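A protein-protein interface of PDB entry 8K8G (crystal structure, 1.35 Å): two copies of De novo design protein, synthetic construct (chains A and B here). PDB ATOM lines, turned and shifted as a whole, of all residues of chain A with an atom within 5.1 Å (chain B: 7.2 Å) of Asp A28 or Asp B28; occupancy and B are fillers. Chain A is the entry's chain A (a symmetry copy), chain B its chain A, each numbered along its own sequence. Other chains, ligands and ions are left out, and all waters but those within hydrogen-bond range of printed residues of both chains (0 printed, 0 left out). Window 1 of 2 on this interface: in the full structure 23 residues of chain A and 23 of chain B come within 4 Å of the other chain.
N of Asp B28 lies within hydrogen-bond range of O of Asp A28 (2.9 Å).
The side-chain carboxylate of Asp B28 is in hydrogen-bond range of the side-chain hydroxyl of Thr B183, 3.1 Å away.
The guanidinium group (NH1) of Arg A200 is in salt-bridge range of the side-chain carboxylate (OD2) of Asp A28.
The guanidinium group of Arg B200 is in salt-bridge range of the side-chain carboxylate of Asp B28 (2.9 Å).
The backbone carbonyl oxygen (O) of Thr B183 lies within hydrogen-bond range of the backbone NH (N) of Leu B29, at 2.8 Å.
N of Leu A29 sits at hydrogen-bond distance from O of Thr A183 (2.8 Å).
OD1 of Asp A28 is in hydrogen-bond range of OG1 of Thr A183, 3.1 Å away.
Leu A26 touches Pro B30.
Glu A27 touches Leu B29.
Asp A28 touches Glu B27 (O to CA, 3.3 Å).
NH1 of Arg B200 touches CB of Asp A28, 3.7 Å away.
OE2 of Glu B27 touches CD2 of Leu A29, 3.4 Å away.
CD of Pro A30 touches O of Leu B26, 3.5 Å away.
Ala A196 touches Arg B200 (CB to NH2, 3.5 Å).
CB of Asp B28 touches NH1 of Arg A200, 3.7 Å away.
Ala B196 touches Arg A200 (CB to NH2, 3.5 Å).
CG of Arg A200 touches CG of Arg B200, at 3.4 Å.
Of chain B, only Glu B27, Asp B28 and Arg B200 come within 4 Å of Asp A28.
Asp B28 touches just these residues of chain A: Glu A27 (3.3 Å), Asp A28 (2.6 Å) and Arg A200 (3.7 Å).
Of the printed residues of chain B, Arg A200 touches Asp B28, Ala B196, Ala B197 and Arg B200.
Printed residues of chain A within 4 Å of Leu B26: Pro A30 (3.5 Å).
Of the printed residues of chain A, Pro B30 touches Leu A26.
Ile B184 touches none of the printed residues of chain A.
Hydrophobic or aromatic side chains of chain A within 4 Å of the printed part of chain B: Leu A29, Pro A30 and Ala A196.
Of the 15 printed residues of chain B, 8 touch a printed residue of chain A.
Hydrophobic or aromatic side chains of chain B within 4 Å of the printed part of chain A: Leu B29, Pro B30, Ala B196 and Ala B197.
Glu A27 touches Asp B28, and with the chains exchanged Asp A28 touches Glu B27.
Asp A28 touches Arg B200, and with the chains exchanged Arg A200 touches Asp B28.
Ala A196 touches Arg B200, and with the chains exchanged Arg A200 touches Ala B196.
Arg B200 touches its own counterpart, Arg A200.
8 positions are printed for both chains.
Of the 13 pairs that touch across the chains among the printed residues, 12 have their exchanged pair printed and touching as well.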
ATOM      1  N   LEU A  26      33.381   7.928 -15.753  1.00  0.00           N
ATOM      2  CA  LEU A  26      32.072   7.394 -16.098  1.00  0.00           C
ATOM      3  C   LEU A  26      31.296   8.440 -16.888  1.00  0.00           C
ATOM      4  O   LEU A  26      31.175   9.596 -16.469  1.00  0.00           O
ATOM      5  CB  LEU A  26      31.342   6.862 -14.856  1.00  0.00           C
ATOM      6  CG  LEU A  26      29.873   6.452 -14.961  1.00  0.00           C
ATOM      7  CD1 LEU A  26      29.747   5.217 -15.863  1.00  0.00           C
ATOM      8  CD2 LEU A  26      29.326   6.104 -13.590  1.00  0.00           C
ATOM      9  N   GLU A  27      30.812   8.034 -18.055  1.00  0.00           N
ATOM     10  CA  GLU A  27      30.083   8.884 -18.971  1.00  0.00           C
ATOM     11  C   GLU A  27      28.764   8.199 -19.289  1.00  0.00           C
ATOM     12  O   GLU A  27      28.665   6.969 -19.273  1.00  0.00           O
ATOM     13  CB  GLU A  27      30.929   9.075 -20.240  1.00  0.00           C
ATOM     14  CG  GLU A  27      30.402  10.019 -21.275  1.00  0.00           C
ATOM     15  CD  GLU A  27      31.377  10.196 -22.434  1.00  0.00           C
ATOM     16  OE1 GLU A  27      32.337   9.407 -22.551  1.00  0.00           O
ATOM     17  OE2 GLU A  27      31.166  11.123 -23.240  1.00  0.00           O
ATOM     18  N   ASP A  28      27.736   8.999 -19.526  1.00  0.00           N
ATOM     19  CA  ASP A  28      26.462   8.471 -19.991  1.00  0.00           C
ATOM     20  C   ASP A  28      26.051   9.273 -21.208  1.00  0.00           C
ATOM     21  O   ASP A  28      26.021  10.506 -21.174  1.00  0.00           O
ATOM     22  CB  ASP A  28      25.421   8.489 -18.874  1.00  0.00           C
ATOM     23  CG  ASP A  28      25.945   7.829 -17.596  1.00  0.00           C
ATOM     24  OD1 ASP A  28      26.373   6.655 -17.633  1.00  0.00           O
ATOM     25  OD2 ASP A  28      25.930   8.467 -16.530  1.00  0.00           O
ATOM     26  N   LEU A  29      25.791   8.564 -22.302  1.00  0.00           N
ATOM     27  CA  LEU A  29      25.499   9.206 -23.564  1.00  0.00           C
ATOM     28  C   LEU A  29      24.158   8.729 -24.100  1.00  0.00           C
ATOM     29  O   LEU A  29      23.875   7.528 -24.079  1.00  0.00           O
ATOM     30  CB  LEU A  29      26.574   8.879 -24.604  1.00  0.00           C
ATOM     31  CG  LEU A  29      27.960   9.502 -24.411  1.00  0.00           C
ATOM     32  CD1 LEU A  29      28.851   9.219 -25.618  1.00  0.00           C
ATOM     33  CD2 LEU A  29      27.880  11.006 -24.127  1.00  0.00           C
ATOM     34  N   PRO A  30      23.329   9.636 -24.588  1.00  0.00           N
ATOM     35  CA  PRO A  30      22.070   9.233 -25.219  1.00  0.00           C
ATOM     36  C   PRO A  30      22.269   8.852 -26.675  1.00  0.00           C
ATOM     37  O   PRO A  30      23.156   9.360 -27.359  1.00  0.00           O
ATOM     38  CB  PRO A  30      21.222  10.505 -25.124  1.00  0.00           C
ATOM     39  CG  PRO A  30      22.258  11.642 -25.162  1.00  0.00           C
ATOM     40  CD  PRO A  30      23.463  11.097 -24.439  1.00  0.00           C
ATOM     41  N   THR A 183      27.907   4.400 -20.543  1.00  0.00           N
ATOM     42  CA  THR A 183      26.576   3.837 -20.708  1.00  0.00           C
ATOM     43  C   THR A 183      25.898   4.536 -21.880  1.00  0.00           C
ATOM     44  O   THR A 183      26.027   5.750 -22.064  1.00  0.00           O
ATOM     45  CB  THR A 183      25.764   4.031 -19.426  1.00  0.00           C
ATOM     46  OG1 THR A 183      26.551   3.646 -18.291  1.00  0.00           O
ATOM     47  CG2 THR A 183      24.542   3.164 -19.443  1.00  0.00           C
ATOM     48  N   ALA A 196      21.279   2.732 -16.417  1.00  0.00           N
ATOM     49  CA  ALA A 196      22.121   3.883 -16.119  1.00  0.00           C
ATOM     50  C   ALA A 196      21.984   4.308 -14.663  1.00  0.00           C
ATOM     51  O   ALA A 196      22.986   4.640 -14.017  1.00  0.00           O
ATOM     52  CB  ALA A 196      21.766   5.033 -17.056  1.00  0.00           C
ATOM     53  N   ARG A 200      25.054   4.370 -11.946  1.00  0.00           N
ATOM     54  CA  ARG A 200      25.391   5.592 -11.216  1.00  0.00           C
ATOM     55  C   ARG A 200      25.307   5.382  -9.711  1.00  0.00           C
ATOM     56  O   ARG A 200      26.141   5.895  -8.962  1.00  0.00           O
ATOM     57  CB  ARG A 200      24.466   6.740 -11.619  1.00  0.00           C
ATOM     58  CG  ARG A 200      24.553   7.174 -13.058  1.00  0.00           C
ATOM     59  CD  ARG A 200      25.948   7.427 -13.548  1.00  0.00           C
ATOM     60  NE  ARG A 200      26.688   8.404 -12.764  1.00  0.00           N
ATOM     61  CZ  ARG A 200      27.655   9.166 -13.257  1.00  0.00           C
ATOM     62  NH1 ARG A 200      27.917   9.200 -14.555  1.00  0.00           N
ATOM     63  NH2 ARG A 200      28.381   9.909 -12.429  1.00  0.00           N
ATOM     64  N   LEU B  26      19.599  13.152 -21.884  1.00  0.00           N
ATOM     65  CA  LEU B  26      20.350  13.265 -20.642  1.00  0.00           C
ATOM     66  C   LEU B  26      21.744  12.685 -20.844  1.00  0.00           C
ATOM     67  O   LEU B  26      21.903  11.557 -21.323  1.00  0.00           O
ATOM     68  CB  LEU B  26      19.572  12.660 -19.464  1.00  0.00           C
ATOM     69  CG  LEU B  26      20.265  12.485 -18.113  1.00  0.00           C
ATOM     70  CD1 LEU B  26      20.580  13.863 -17.514  1.00  0.00           C
ATOM     71  CD2 LEU B  26      19.360  11.739 -17.151  1.00  0.00           C
ATOM     72  N   GLU B  27      22.750  13.485 -20.517  1.00  0.00           N
ATOM     73  CA  GLU B  27      24.146  13.138 -20.671  1.00  0.00           C
ATOM     74  C   GLU B  27      24.826  13.341 -19.327  1.00  0.00           C
ATOM     75  O   GLU B  27      24.417  14.188 -18.528  1.00  0.00           O
ATOM     76  CB  GLU B  27      24.761  14.048 -21.747  1.00  0.00           C
ATOM     77  CG  GLU B  27      26.178  13.775 -22.141  1.00  0.00           C
ATOM     78  CD  GLU B  27      26.636  14.678 -23.282  1.00  0.00           C
ATOM     79  OE1 GLU B  27      25.942  15.668 -23.594  1.00  0.00           O
ATOM     80  OE2 GLU B  27      27.706  14.399 -23.857  1.00  0.00           O
ATOM     81  N   ASP B  28      25.832  12.525 -19.056  1.00  0.00           N
ATOM     82  CA  ASP B  28      26.660  12.716 -17.874  1.00  0.00           C
ATOM     83  C   ASP B  28      28.107  12.695 -18.321  1.00  0.00           C
ATOM     84  O   ASP B  28      28.545  11.769 -19.009  1.00  0.00           O
ATOM     85  CB  ASP B  28      26.340  11.672 -16.806  1.00  0.00           C
ATOM     86  CG  ASP B  28      24.840  11.596 -16.516  1.00  0.00           C
ATOM     87  OD1 ASP B  28      24.220  12.625 -16.170  1.00  0.00           O
ATOM     88  OD2 ASP B  28      24.254  10.505 -16.617  1.00  0.00           O
ATOM     89  N   LEU B  29      28.832  13.754 -17.971  1.00  0.00           N
ATOM     90  CA  LEU B  29      30.193  13.918 -18.427  1.00  0.00           C
ATOM     91  C   LEU B  29      31.129  14.091 -17.241  1.00  0.00           C
ATOM     92  O   LEU B  29      30.823  14.847 -16.315  1.00  0.00           O
ATOM     93  CB  LEU B  29      30.323  15.154 -19.322  1.00  0.00           C
ATOM     94  CG  LEU B  29      29.683  15.093 -20.712  1.00  0.00           C
ATOM     95  CD1 LEU B  29      30.054  16.328 -21.531  1.00  0.00           C
ATOM     96  CD2 LEU B  29      30.051  13.807 -21.459  1.00  0.00           C
ATOM     97  N   PRO B  30      32.266  13.415 -17.247  1.00  0.00           N
ATOM     98  CA  PRO B  30      33.260  13.618 -16.190  1.00  0.00           C
ATOM     99  C   PRO B  30      34.145  14.817 -16.477  1.00  0.00           C
ATOM    100  O   PRO B  30      34.401  15.171 -17.626  1.00  0.00           O
ATOM    101  CB  PRO B  30      34.088  12.331 -16.253  1.00  0.00           C
ATOM    102  CG  PRO B  30      33.995  11.905 -17.728  1.00  0.00           C
ATOM    103  CD  PRO B  30      32.613  12.317 -18.168  1.00  0.00           C
ATOM    104  N   VAL B 181      20.174  17.811 -21.087  1.00  0.00           N
ATOM    105  CA  VAL B 181      20.577  17.975 -19.695  1.00  0.00           C
ATOM    106  C   VAL B 181      21.923  17.293 -19.556  1.00  0.00           C
ATOM    107  O   VAL B 181      22.072  16.134 -19.944  1.00  0.00           O
ATOM    108  CB  VAL B 181      19.569  17.325 -18.734  1.00  0.00           C
ATOM    109  CG1 VAL B 181      20.052  17.441 -17.290  1.00  0.00           C
ATOM    110  CG2 VAL B 181      18.177  17.940 -18.917  1.00  0.00           C
ATOM    111  N   VAL B 182      22.908  18.007 -19.009  1.00  0.00           N
ATOM    112  CA  VAL B 182      24.282  17.499 -18.898  1.00  0.00           C
ATOM    113  C   VAL B 182      24.727  17.640 -17.448  1.00  0.00           C
ATOM    114  O   VAL B 182      24.941  18.760 -16.971  1.00  0.00           O
ATOM    115  CB  VAL B 182      25.261  18.242 -19.822  1.00  0.00           C
ATOM    116  CG1 VAL B 182      26.623  17.563 -19.832  1.00  0.00           C
ATOM    117  CG2 VAL B 182      24.716  18.375 -21.232  1.00  0.00           C
ATOM    118  N   THR B 183      24.860  16.519 -16.751  1.00  0.00           N
ATOM    119  CA  THR B 183      25.472  16.540 -15.432  1.00  0.00           C
ATOM    120  C   THR B 183      26.984  16.470 -15.600  1.00  0.00           C
ATOM    121  O   THR B 183      27.501  15.743 -16.453  1.00  0.00           O
ATOM    122  CB  THR B 183      24.969  15.355 -14.604  1.00  0.00           C
ATOM    123  OG1 THR B 183      23.543  15.258 -14.712  1.00  0.00           O
ATOM    124  CG2 THR B 183      25.300  15.550 -13.155  1.00  0.00           C
ATOM    125  N   ILE B 184      27.698  17.274 -14.817  1.00  0.00           N
ATOM    126  CA  ILE B 184      29.156  17.302 -14.854  1.00  0.00           C
ATOM    127  C   ILE B 184      29.664  16.957 -13.464  1.00  0.00           C
ATOM    128  O   ILE B 184      29.235  17.568 -12.479  1.00  0.00           O
ATOM    129  CB  ILE B 184      29.677  18.688 -15.261  1.00  0.00           C
ATOM    130  CG1 ILE B 184      29.052  19.161 -16.573  1.00  0.00           C
ATOM    131  CG2 ILE B 184      31.200  18.687 -15.287  1.00  0.00           C
ATOM    132  CD1 ILE B 184      29.498  18.394 -17.744  1.00  0.00           C
ATOM    133  N   GLY B 185      30.563  15.981 -13.383  1.00  0.00           N
ATOM    134  CA  GLY B 185      31.076  15.592 -12.086  1.00  0.00           C
ATOM    135  C   GLY B 185      32.565  15.364 -12.082  1.00  0.00           C
ATOM    136  O   GLY B 185      33.130  14.789 -13.024  1.00  0.00           O
ATOM    137  N   LEU B 195      24.713  13.352  -6.844  1.00  0.00           N
ATOM    138  CA  LEU B 195      23.809  14.154  -7.661  1.00  0.00           C
ATOM    139  C   LEU B 195      23.473  13.441  -8.963  1.00  0.00           C
ATOM    140  O   LEU B 195      22.310  13.362  -9.359  1.00  0.00           O
ATOM    141  CB  LEU B 195      24.431  15.519  -7.936  1.00  0.00           C
ATOM    142  CG  LEU B 195      23.597  16.447  -8.815  1.00  0.00           C
ATOM    143  CD1 LEU B 195      22.220  16.645  -8.204  1.00  0.00           C
ATOM    144  CD2 LEU B 195      24.315  17.769  -8.967  1.00  0.00           C
ATOM    145  N   ALA B 196      24.489  12.910  -9.639  1.00  0.00           N
ATOM    146  CA  ALA B 196      24.240  12.206 -10.890  1.00  0.00           C
ATOM    147  C   ALA B 196      23.338  10.998 -10.678  1.00  0.00           C
ATOM    148  O   ALA B 196      22.440  10.744 -11.491  1.00  0.00           O
ATOM    149  CB  ALA B 196      25.568  11.791 -11.515  1.00  0.00           C
ATOM    150  N   ALA B 197      23.552  10.253  -9.583  1.00  0.00           N
ATOM    151  CA  ALA B 197      22.702   9.094  -9.309  1.00  0.00           C
ATOM    152  C   ALA B 197      21.267   9.520  -9.049  1.00  0.00           C
ATOM    153  O   ALA B 197      20.323   8.868  -9.499  1.00  0.00           O
ATOM    154  CB  ALA B 197      23.248   8.311  -8.119  1.00  0.00           C
ATOM    155  N   ILE B 199      19.749  12.240 -10.222  1.00  0.00           N
ATOM    156  CA  ILE B 199      19.133  12.673 -11.472  1.00  0.00           C
ATOM    157  C   ILE B 199      18.779  11.481 -12.358  1.00  0.00           C
ATOM    158  O   ILE B 199      17.707  11.449 -12.973  1.00  0.00           O
ATOM    159  CB  ILE B 199      20.043  13.693 -12.178  1.00  0.00           C
ATOM    160  CG1 ILE B 199      20.038  15.001 -11.387  1.00  0.00           C
ATOM    161  CG2 ILE B 199      19.575  13.962 -13.575  1.00  0.00           C
ATOM    162  CD1 ILE B 199      21.086  15.995 -11.840  1.00  0.00           C
ATOM    163  N   ARG B 200      19.668  10.483 -12.431  1.00  0.00           N
ATOM    164  CA  ARG B 200      19.372   9.293 -13.227  1.00  0.00           C
ATOM    165  C   ARG B 200      18.173   8.536 -12.673  1.00  0.00           C
ATOM    166  O   ARG B 200      17.348   8.029 -13.436  1.00  0.00           O
ATOM    167  CB  ARG B 200      20.580   8.359 -13.280  1.00  0.00           C
ATOM    168  CG  ARG B 200      21.807   8.916 -13.951  1.00  0.00           C
ATOM    169  CD  ARG B 200      21.557   9.526 -15.298  1.00  0.00           C
ATOM    170  NE  ARG B 200      20.922   8.628 -16.251  1.00  0.00           N
ATOM    171  CZ  ARG B 200      21.080   8.714 -17.565  1.00  0.00           C
ATOM    172  NH1 ARG B 200      21.962   9.542 -18.103  1.00  0.00           N
ATOM    173  NH2 ARG B 200      20.334   7.955 -18.359  1.00  0.00           N
